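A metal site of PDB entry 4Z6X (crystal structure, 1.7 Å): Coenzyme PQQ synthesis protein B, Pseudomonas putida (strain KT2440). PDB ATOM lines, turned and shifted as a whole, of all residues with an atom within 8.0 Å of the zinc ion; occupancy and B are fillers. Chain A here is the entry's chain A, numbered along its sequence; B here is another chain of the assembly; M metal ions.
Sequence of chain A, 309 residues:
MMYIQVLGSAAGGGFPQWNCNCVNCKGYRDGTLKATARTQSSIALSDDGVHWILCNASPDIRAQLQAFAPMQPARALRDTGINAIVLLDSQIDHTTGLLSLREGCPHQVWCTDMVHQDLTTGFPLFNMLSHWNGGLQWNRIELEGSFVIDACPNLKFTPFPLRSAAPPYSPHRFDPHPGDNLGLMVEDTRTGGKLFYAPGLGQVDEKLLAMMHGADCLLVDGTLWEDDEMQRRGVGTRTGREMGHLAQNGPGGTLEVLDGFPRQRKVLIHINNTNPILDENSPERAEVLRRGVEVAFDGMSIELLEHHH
ND2 of Asn 24 lies within hydrogen-bond range of O of Asn 273, at 3.0 Å.
The side-chain amide nitrogen (ND2) of Asn 273 sits at hydrogen-bond distance from the side-chain amide oxygen (OE1) of Gln 17, 3.2 Å away.
The side-chain sulfur of Cys 22 lies close to the backbone NH of Asn 24.
SG of Cys 25 lies close to N of Gln 17 (3.5 Å).
The guanidinium group of Arg 29 is in hydrogen-bond range of the backbone carbonyl oxygen of Cys 20 (2.8 Å).
The side-chain amide oxygen (OD1) of Asn 273 binds the zinc ion (2.0 Å).
The zinc ion is bound by SG of Cys 22, at 2.3 Å.
SG of Cys 25 binds the zinc ion, at 2.3 Å.
SG of Cys 20 binds the zinc ion.
The zinc ion has four donor atoms within binding distance.
Within 4 Å of the zinc ion: Cys 20, Cys 22, Cys 25 and Asn 273.
Along chain A the residues within 4 Å of the zinc ion span positions 20 to 273.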
ATOM      1  N   GLY A  14      26.261  -2.100 -11.215  1.00  0.00           N
ATOM      2  CA  GLY A  14      26.237  -3.402 -10.595  1.00  0.00           C
ATOM      3  C   GLY A  14      24.812  -3.805 -10.189  1.00  0.00           C
ATOM      4  O   GLY A  14      23.816  -3.150 -10.544  1.00  0.00           O
ATOM      5  N   PHE A  15      24.714  -4.905  -9.467  1.00  0.00           N
ATOM      6  CA  PHE A  15      23.414  -5.377  -8.990  1.00  0.00           C
ATOM      7  C   PHE A  15      23.531  -5.961  -7.602  1.00  0.00           C
ATOM      8  O   PHE A  15      24.300  -6.891  -7.412  1.00  0.00           O
ATOM      9  CB  PHE A  15      22.813  -6.432  -9.938  1.00  0.00           C
ATOM     10  CG  PHE A  15      21.575  -7.074  -9.373  1.00  0.00           C
ATOM     11  CD1 PHE A  15      20.437  -6.314  -9.153  1.00  0.00           C
ATOM     12  CD2 PHE A  15      21.566  -8.403  -9.027  1.00  0.00           C
ATOM     13  CE1 PHE A  15      19.293  -6.888  -8.609  1.00  0.00           C
ATOM     14  CE2 PHE A  15      20.429  -8.995  -8.477  1.00  0.00           C
ATOM     15  CZ  PHE A  15      19.291  -8.231  -8.281  1.00  0.00           C
ATOM     16  N   PRO A  16      22.801  -5.409  -6.598  1.00  0.00           N
ATOM     17  CA  PRO A  16      21.954  -4.217  -6.646  1.00  0.00           C
ATOM     18  C   PRO A  16      22.796  -2.954  -6.845  1.00  0.00           C
ATOM     19  O   PRO A  16      23.978  -2.947  -6.512  1.00  0.00           O
ATOM     20  CB  PRO A  16      21.287  -4.211  -5.259  1.00  0.00           C
ATOM     21  CG  PRO A  16      22.307  -4.835  -4.357  1.00  0.00           C
ATOM     22  CD  PRO A  16      22.978  -5.916  -5.228  1.00  0.00           C
ATOM     23  N   GLN A  17      22.188  -1.916  -7.399  1.00  0.00           N
ATOM     24  CA  GLN A  17      22.871  -0.658  -7.580  1.00  0.00           C
ATOM     25  C   GLN A  17      22.661   0.193  -6.324  1.00  0.00           C
ATOM     26  O   GLN A  17      21.555   0.229  -5.764  1.00  0.00           O
ATOM     27  CB  GLN A  17      22.328   0.062  -8.815  1.00  0.00           C
ATOM     28  CG  GLN A  17      22.951   1.444  -9.029  1.00  0.00           C
ATOM     29  CD  GLN A  17      22.594   2.032 -10.372  1.00  0.00           C
ATOM     30  OE1 GLN A  17      22.809   1.402 -11.417  1.00  0.00           O
ATOM     31  NE2 GLN A  17      22.062   3.259 -10.354  1.00  0.00           N
ATOM     32  N   TRP A  18      23.729   0.865  -5.897  1.00  0.00           N
ATOM     33  CA  TRP A  18      23.790   1.509  -4.585  1.00  0.00           C
ATOM     34  C   TRP A  18      22.623   2.455  -4.266  1.00  0.00           C
ATOM     35  O   TRP A  18      22.174   2.518  -3.107  1.00  0.00           O
ATOM     36  CB  TRP A  18      25.121   2.289  -4.457  1.00  0.00           C
ATOM     37  CG  TRP A  18      25.171   3.492  -5.342  1.00  0.00           C
ATOM     38  CD1 TRP A  18      25.430   3.514  -6.699  1.00  0.00           C
ATOM     39  CD2 TRP A  18      24.972   4.846  -4.944  1.00  0.00           C
ATOM     40  NE1 TRP A  18      25.381   4.822  -7.156  1.00  0.00           N
ATOM     41  CE2 TRP A  18      25.113   5.655  -6.094  1.00  0.00           C
ATOM     42  CE3 TRP A  18      24.681   5.459  -3.702  1.00  0.00           C
ATOM     43  CZ2 TRP A  18      24.944   7.054  -6.043  1.00  0.00           C
ATOM     44  CZ3 TRP A  18      24.508   6.849  -3.668  1.00  0.00           C
ATOM     45  CH2 TRP A  18      24.656   7.624  -4.826  1.00  0.00           C
ATOM     46  N   ASN A  19      22.134   3.165  -5.283  1.00  0.00           N
ATOM     47  CA  ASN A  19      21.064   4.153  -5.030  1.00  0.00           C
ATOM     48  C   ASN A  19      19.728   3.747  -5.633  1.00  0.00           C
ATOM     49  O   ASN A  19      18.811   4.578  -5.762  1.00  0.00           O
ATOM     50  CB  ASN A  19      21.461   5.548  -5.559  1.00  0.00           C
ATOM     51  CG  ASN A  19      21.563   5.607  -7.066  1.00  0.00           C
ATOM     52  OD1 ASN A  19      21.794   4.580  -7.708  1.00  0.00           O
ATOM     53  ND2 ASN A  19      21.401   6.797  -7.644  1.00  0.00           N
ATOM     54  N   CYS A  20      19.604   2.468  -5.977  1.00  0.00           N
ATOM     55  CA  CYS A  20      18.418   2.004  -6.725  1.00  0.00           C
ATOM     56  C   CYS A  20      17.479   1.140  -5.898  1.00  0.00           C
ATOM     57  O   CYS A  20      17.916   0.199  -5.224  1.00  0.00           O
ATOM     58  CB  CYS A  20      18.835   1.211  -7.979  1.00  0.00           C
ATOM     59  SG  CYS A  20      17.371   0.851  -9.050  1.00  0.00           S
ATOM     60  N   ASN A  21      16.176   1.448  -5.989  1.00  0.00           N
ATOM     61  CA  ASN A  21      15.147   0.648  -5.319  1.00  0.00           C
ATOM     62  C   ASN A  21      14.109   0.156  -6.283  1.00  0.00           C
ATOM     63  O   ASN A  21      12.938   0.047  -5.944  1.00  0.00           O
ATOM     64  CB  ASN A  21      14.474   1.465  -4.195  1.00  0.00           C
ATOM     65  CG  ASN A  21      15.482   1.887  -3.133  1.00  0.00           C
ATOM     66  OD1 ASN A  21      16.022   1.047  -2.430  1.00  0.00           O
ATOM     67  ND2 ASN A  21      15.761   3.192  -3.056  1.00  0.00           N
ATOM     68  N   CYS A  22      14.548  -0.192  -7.484  1.00  0.00           N
ATOM     69  CA  CYS A  22      13.644  -0.760  -8.501  1.00  0.00           C
ATOM     70  C   CYS A  22      13.196  -2.130  -8.029  1.00  0.00           C
ATOM     71  O   CYS A  22      13.697  -2.631  -7.024  1.00  0.00           O
ATOM     72  CB  CYS A  22      14.333  -0.838  -9.859  1.00  0.00           C
ATOM     73  SG  CYS A  22      15.531  -2.236 -10.094  1.00  0.00           S
ATOM     74  N   VAL A  23      12.240  -2.721  -8.738  1.00  0.00           N
ATOM     75  CA  VAL A  23      11.702  -4.011  -8.350  1.00  0.00           C
ATOM     76  C   VAL A  23      12.787  -5.039  -8.019  1.00  0.00           C
ATOM     77  O   VAL A  23      12.686  -5.758  -7.013  1.00  0.00           O
ATOM     78  CB  VAL A  23      10.791  -4.557  -9.456  1.00  0.00           C
ATOM     79  CG1 VAL A  23      10.371  -5.976  -9.148  1.00  0.00           C
ATOM     80  CG2 VAL A  23       9.577  -3.678  -9.570  1.00  0.00           C
ATOM     81  N   ASN A  24      13.826  -5.091  -8.851  1.00  0.00           N
ATOM     82  CA  ASN A  24      14.920  -6.045  -8.671  1.00  0.00           C
ATOM     83  C   ASN A  24      15.831  -5.735  -7.487  1.00  0.00           C
ATOM     84  O   ASN A  24      16.146  -6.623  -6.683  1.00  0.00           O
ATOM     85  CB  ASN A  24      15.773  -6.110  -9.939  1.00  0.00           C
ATOM     86  CG  ASN A  24      15.213  -7.076 -10.974  1.00  0.00           C
ATOM     87  OD1 ASN A  24      14.251  -7.802 -10.708  1.00  0.00           O
ATOM     88  ND2 ASN A  24      15.832  -7.095 -12.150  1.00  0.00           N
ATOM     89  N   CYS A  25      16.276  -4.478  -7.392  1.00  0.00           N
ATOM     90  CA  CYS A  25      17.203  -4.094  -6.338  1.00  0.00           C
ATOM     91  C   CYS A  25      16.513  -4.184  -4.968  1.00  0.00           C
ATOM     92  O   CYS A  25      17.080  -4.710  -4.013  1.00  0.00           O
ATOM     93  CB  CYS A  25      17.758  -2.688  -6.593  1.00  0.00           C
ATOM     94  SG  CYS A  25      18.866  -2.653  -8.074  1.00  0.00           S
ATOM     95  N   LYS A  26      15.284  -3.693  -4.869  1.00  0.00           N
ATOM     96  CA  LYS A  26      14.593  -3.733  -3.579  1.00  0.00           C
ATOM     97  C   LYS A  26      14.243  -5.172  -3.222  1.00  0.00           C
ATOM     98  O   LYS A  26      14.366  -5.586  -2.065  1.00  0.00           O
ATOM     99  CB  LYS A  26      13.333  -2.872  -3.627  1.00  0.00           C
ATOM    100  CG  LYS A  26      12.619  -2.663  -2.292  1.00  0.00           C
ATOM    101  CD  LYS A  26      11.538  -1.600  -2.471  1.00  0.00           C
ATOM    102  CE  LYS A  26      10.806  -1.278  -1.185  1.00  0.00           C
ATOM    103  NZ  LYS A  26      10.055  -2.474  -0.757  1.00  0.00           N
ATOM    104  N   GLY A  27      13.826  -5.935  -4.219  1.00  0.00           N
ATOM    105  CA  GLY A  27      13.503  -7.342  -4.055  1.00  0.00           C
ATOM    106  C   GLY A  27      14.710  -8.133  -3.573  1.00  0.00           C
ATOM    107  O   GLY A  27      14.592  -9.014  -2.735  1.00  0.00           O
ATOM    108  N   ARG A  29      17.328  -6.841  -1.823  1.00  0.00           N
ATOM    109  CA  ARG A  29      17.615  -6.435  -0.453  1.00  0.00           C
ATOM    110  C   ARG A  29      16.579  -6.996   0.525  1.00  0.00           C
ATOM    111  O   ARG A  29      16.938  -7.306   1.654  1.00  0.00           O
ATOM    112  CB  ARG A  29      17.711  -4.907  -0.335  1.00  0.00           C
ATOM    113  CG  ARG A  29      18.887  -4.304  -1.151  1.00  0.00           C
ATOM    114  CD  ARG A  29      19.087  -2.849  -0.763  1.00  0.00           C
ATOM    115  NE  ARG A  29      19.897  -2.152  -1.761  1.00  0.00           N
ATOM    116  CZ  ARG A  29      19.380  -1.484  -2.796  1.00  0.00           C
ATOM    117  NH1 ARG A  29      20.206  -0.908  -3.673  1.00  0.00           N
ATOM    118  NH2 ARG A  29      18.051  -1.412  -2.960  1.00  0.00           N
ATOM    119  N   ARG A 233      10.683   0.648 -15.224  1.00  0.00           N
ATOM    120  CA  ARG A 233      11.050   0.478 -13.824  1.00  0.00           C
ATOM    121  C   ARG A 233      11.046   1.784 -13.041  1.00  0.00           C
ATOM    122  O   ARG A 233      11.117   1.770 -11.802  1.00  0.00           O
ATOM    123  CB  ARG A 233      12.444  -0.135 -13.733  1.00  0.00           C
ATOM    124  CG  ARG A 233      12.644  -1.389 -14.543  1.00  0.00           C
ATOM    125  CD  ARG A 233      11.730  -2.484 -14.089  1.00  0.00           C
ATOM    126  NE  ARG A 233      12.364  -3.787 -14.243  1.00  0.00           N
ATOM    127  CZ  ARG A 233      11.756  -4.940 -13.961  1.00  0.00           C
ATOM    128  NH1 ARG A 233      12.387  -6.101 -14.103  1.00  0.00           N
ATOM    129  NH2 ARG A 233      10.485  -4.915 -13.548  1.00  0.00           N
ATOM    130  N   VAL A 235      13.295   4.288 -13.112  1.00  0.00           N
ATOM    131  CA  VAL A 235      14.587   4.735 -12.564  1.00  0.00           C
ATOM    132  C   VAL A 235      15.511   5.441 -13.549  1.00  0.00           C
ATOM    133  O   VAL A 235      16.670   5.715 -13.215  1.00  0.00           O
ATOM    134  CB  VAL A 235      15.362   3.551 -11.946  1.00  0.00           C
ATOM    135  CG1 VAL A 235      14.687   3.082 -10.681  1.00  0.00           C
ATOM    136  CG2 VAL A 235      15.503   2.429 -12.953  1.00  0.00           C
ATOM    137  N   ASN A 272      21.865  -5.122 -16.845  1.00  0.00           N
ATOM    138  CA  ASN A 272      21.469  -4.006 -15.955  1.00  0.00           C
ATOM    139  C   ASN A 272      20.659  -4.478 -14.758  1.00  0.00           C
ATOM    140  O   ASN A 272      19.956  -5.486 -14.840  1.00  0.00           O
ATOM    141  CB  ASN A 272      20.657  -2.947 -16.709  1.00  0.00           C
ATOM    142  CG  ASN A 272      20.785  -1.571 -16.049  1.00  0.00           C
ATOM    143  OD1 ASN A 272      21.893  -1.157 -15.712  1.00  0.00           O
ATOM    144  ND2 ASN A 272      19.677  -0.894 -15.842  1.00  0.00           N
ATOM    145  N   ASN A 273      20.747  -3.737 -13.647  1.00  0.00           N
ATOM    146  CA  ASN A 273      20.048  -4.123 -12.439  1.00  0.00           C
ATOM    147  C   ASN A 273      18.548  -4.213 -12.653  1.00  0.00           C
ATOM    148  O   ASN A 273      17.870  -4.918 -11.922  1.00  0.00           O
ATOM    149  CB  ASN A 273      20.367  -3.141 -11.296  1.00  0.00           C
ATOM    150  CG  ASN A 273      19.785  -1.745 -11.540  1.00  0.00           C
ATOM    151  OD1 ASN A 273      18.604  -1.475 -11.256  1.00  0.00           O
ATOM    152  ND2 ASN A 273      20.621  -0.847 -12.062  1.00  0.00           N
ATOM    153  N   THR A 274      18.031  -3.528 -13.674  1.00  0.00           N
ATOM    154  CA  THR A 274      16.582  -3.506 -13.955  1.00  0.00           C
ATOM    155  C   THR A 274      16.091  -4.715 -14.765  1.00  0.00           C
ATOM    156  O   THR A 274      14.883  -4.918 -14.941  1.00  0.00           O
ATOM    157  CB  THR A 274      16.184  -2.246 -14.747  1.00  0.00           C
ATOM    158  OG1 THR A 274      17.020  -2.118 -15.911  1.00  0.00           O
ATOM    159  CG2 THR A 274      16.301  -1.003 -13.873  1.00  0.00           C
ATOM    160  N   ASN A 275      17.029  -5.509 -15.272  1.00  0.00           N
ATOM    161  CA  ASN A 275      16.683  -6.538 -16.261  1.00  0.00           C
ATOM    162  C   ASN A 275      16.010  -7.759 -15.623  1.00  0.00           C
ATOM    163  O   ASN A 275      16.601  -8.430 -14.775  1.00  0.00           O
ATOM    164  CB  ASN A 275      17.946  -6.946 -17.044  1.00  0.00           C
ATOM    165  CG  ASN A 275      17.610  -7.745 -18.294  1.00  0.00           C
ATOM    166  OD1 ASN A 275      16.627  -8.485 -18.322  1.00  0.00           O
ATOM    167  ND2 ASN A 275      18.436  -7.609 -19.333  1.00  0.00           N
ATOM    168  N   LEU A 278      17.493 -11.227 -14.536  1.00  0.00           N
ATOM    169  CA  LEU A 278      18.208 -11.401 -13.275  1.00  0.00           C
ATOM    170  C   LEU A 278      17.348 -12.153 -12.273  1.00  0.00           C
ATOM    171  O   LEU A 278      17.875 -12.812 -11.380  1.00  0.00           O
ATOM    172  CB  LEU A 278      18.609 -10.056 -12.679  1.00  0.00           C
ATOM    173  CG  LEU A 278      19.685  -9.270 -13.411  1.00  0.00           C
ATOM    174  CD1 LEU A 278      19.941  -7.927 -12.676  1.00  0.00           C
ATOM    175  CD2 LEU A 278      20.964 -10.088 -13.455  1.00  0.00           C
ATOM    176  N   LEU B  77      12.278   5.487  -5.556  1.00  0.00           N
ATOM    177  CA  LEU B  77      12.891   4.567  -6.513  1.00  0.00           C
ATOM    178  C   LEU B  77      14.392   4.821  -6.605  1.00  0.00           C
ATOM    179  O   LEU B  77      15.171   3.892  -6.792  1.00  0.00           O
ATOM    180  CB  LEU B  77      12.252   4.708  -7.890  1.00  0.00           C
ATOM    181  CG  LEU B  77      10.901   3.983  -7.939  1.00  0.00           C
ATOM    182  CD1 LEU B  77      10.081   4.414  -9.161  1.00  0.00           C
ATOM    183  CD2 LEU B  77      11.129   2.458  -7.932  1.00  0.00           C
ATOM    184  N   ARG B  78      14.769   6.099  -6.527  1.00  0.00           N
ATOM    185  CA  ARG B  78      16.169   6.492  -6.343  1.00  0.00           C
ATOM    186  C   ARG B  78      16.317   7.085  -4.960  1.00  0.00           C
ATOM    187  O   ARG B  78      15.552   7.968  -4.572  1.00  0.00           O
ATOM    188  CB  ARG B  78      16.612   7.506  -7.392  1.00  0.00           C
ATOM    189  CG  ARG B  78      17.434   6.939  -8.514  1.00  0.00           C
ATOM    190  CD  ARG B  78      16.716   5.841  -9.254  1.00  0.00           C
ATOM    191  NE  ARG B  78      17.459   5.457 -10.444  1.00  0.00           N
ATOM    192  CZ  ARG B  78      18.572   4.716 -10.428  1.00  0.00           C
ATOM    193  NH1 ARG B  78      19.073   4.291  -9.278  1.00  0.00           N
ATOM    194  NH2 ARG B  78      19.180   4.407 -11.564  1.00  0.00           N
HETATM  195 ZN    ZN M   1      17.586  -1.446  -9.522  1.00  0.00          ZN
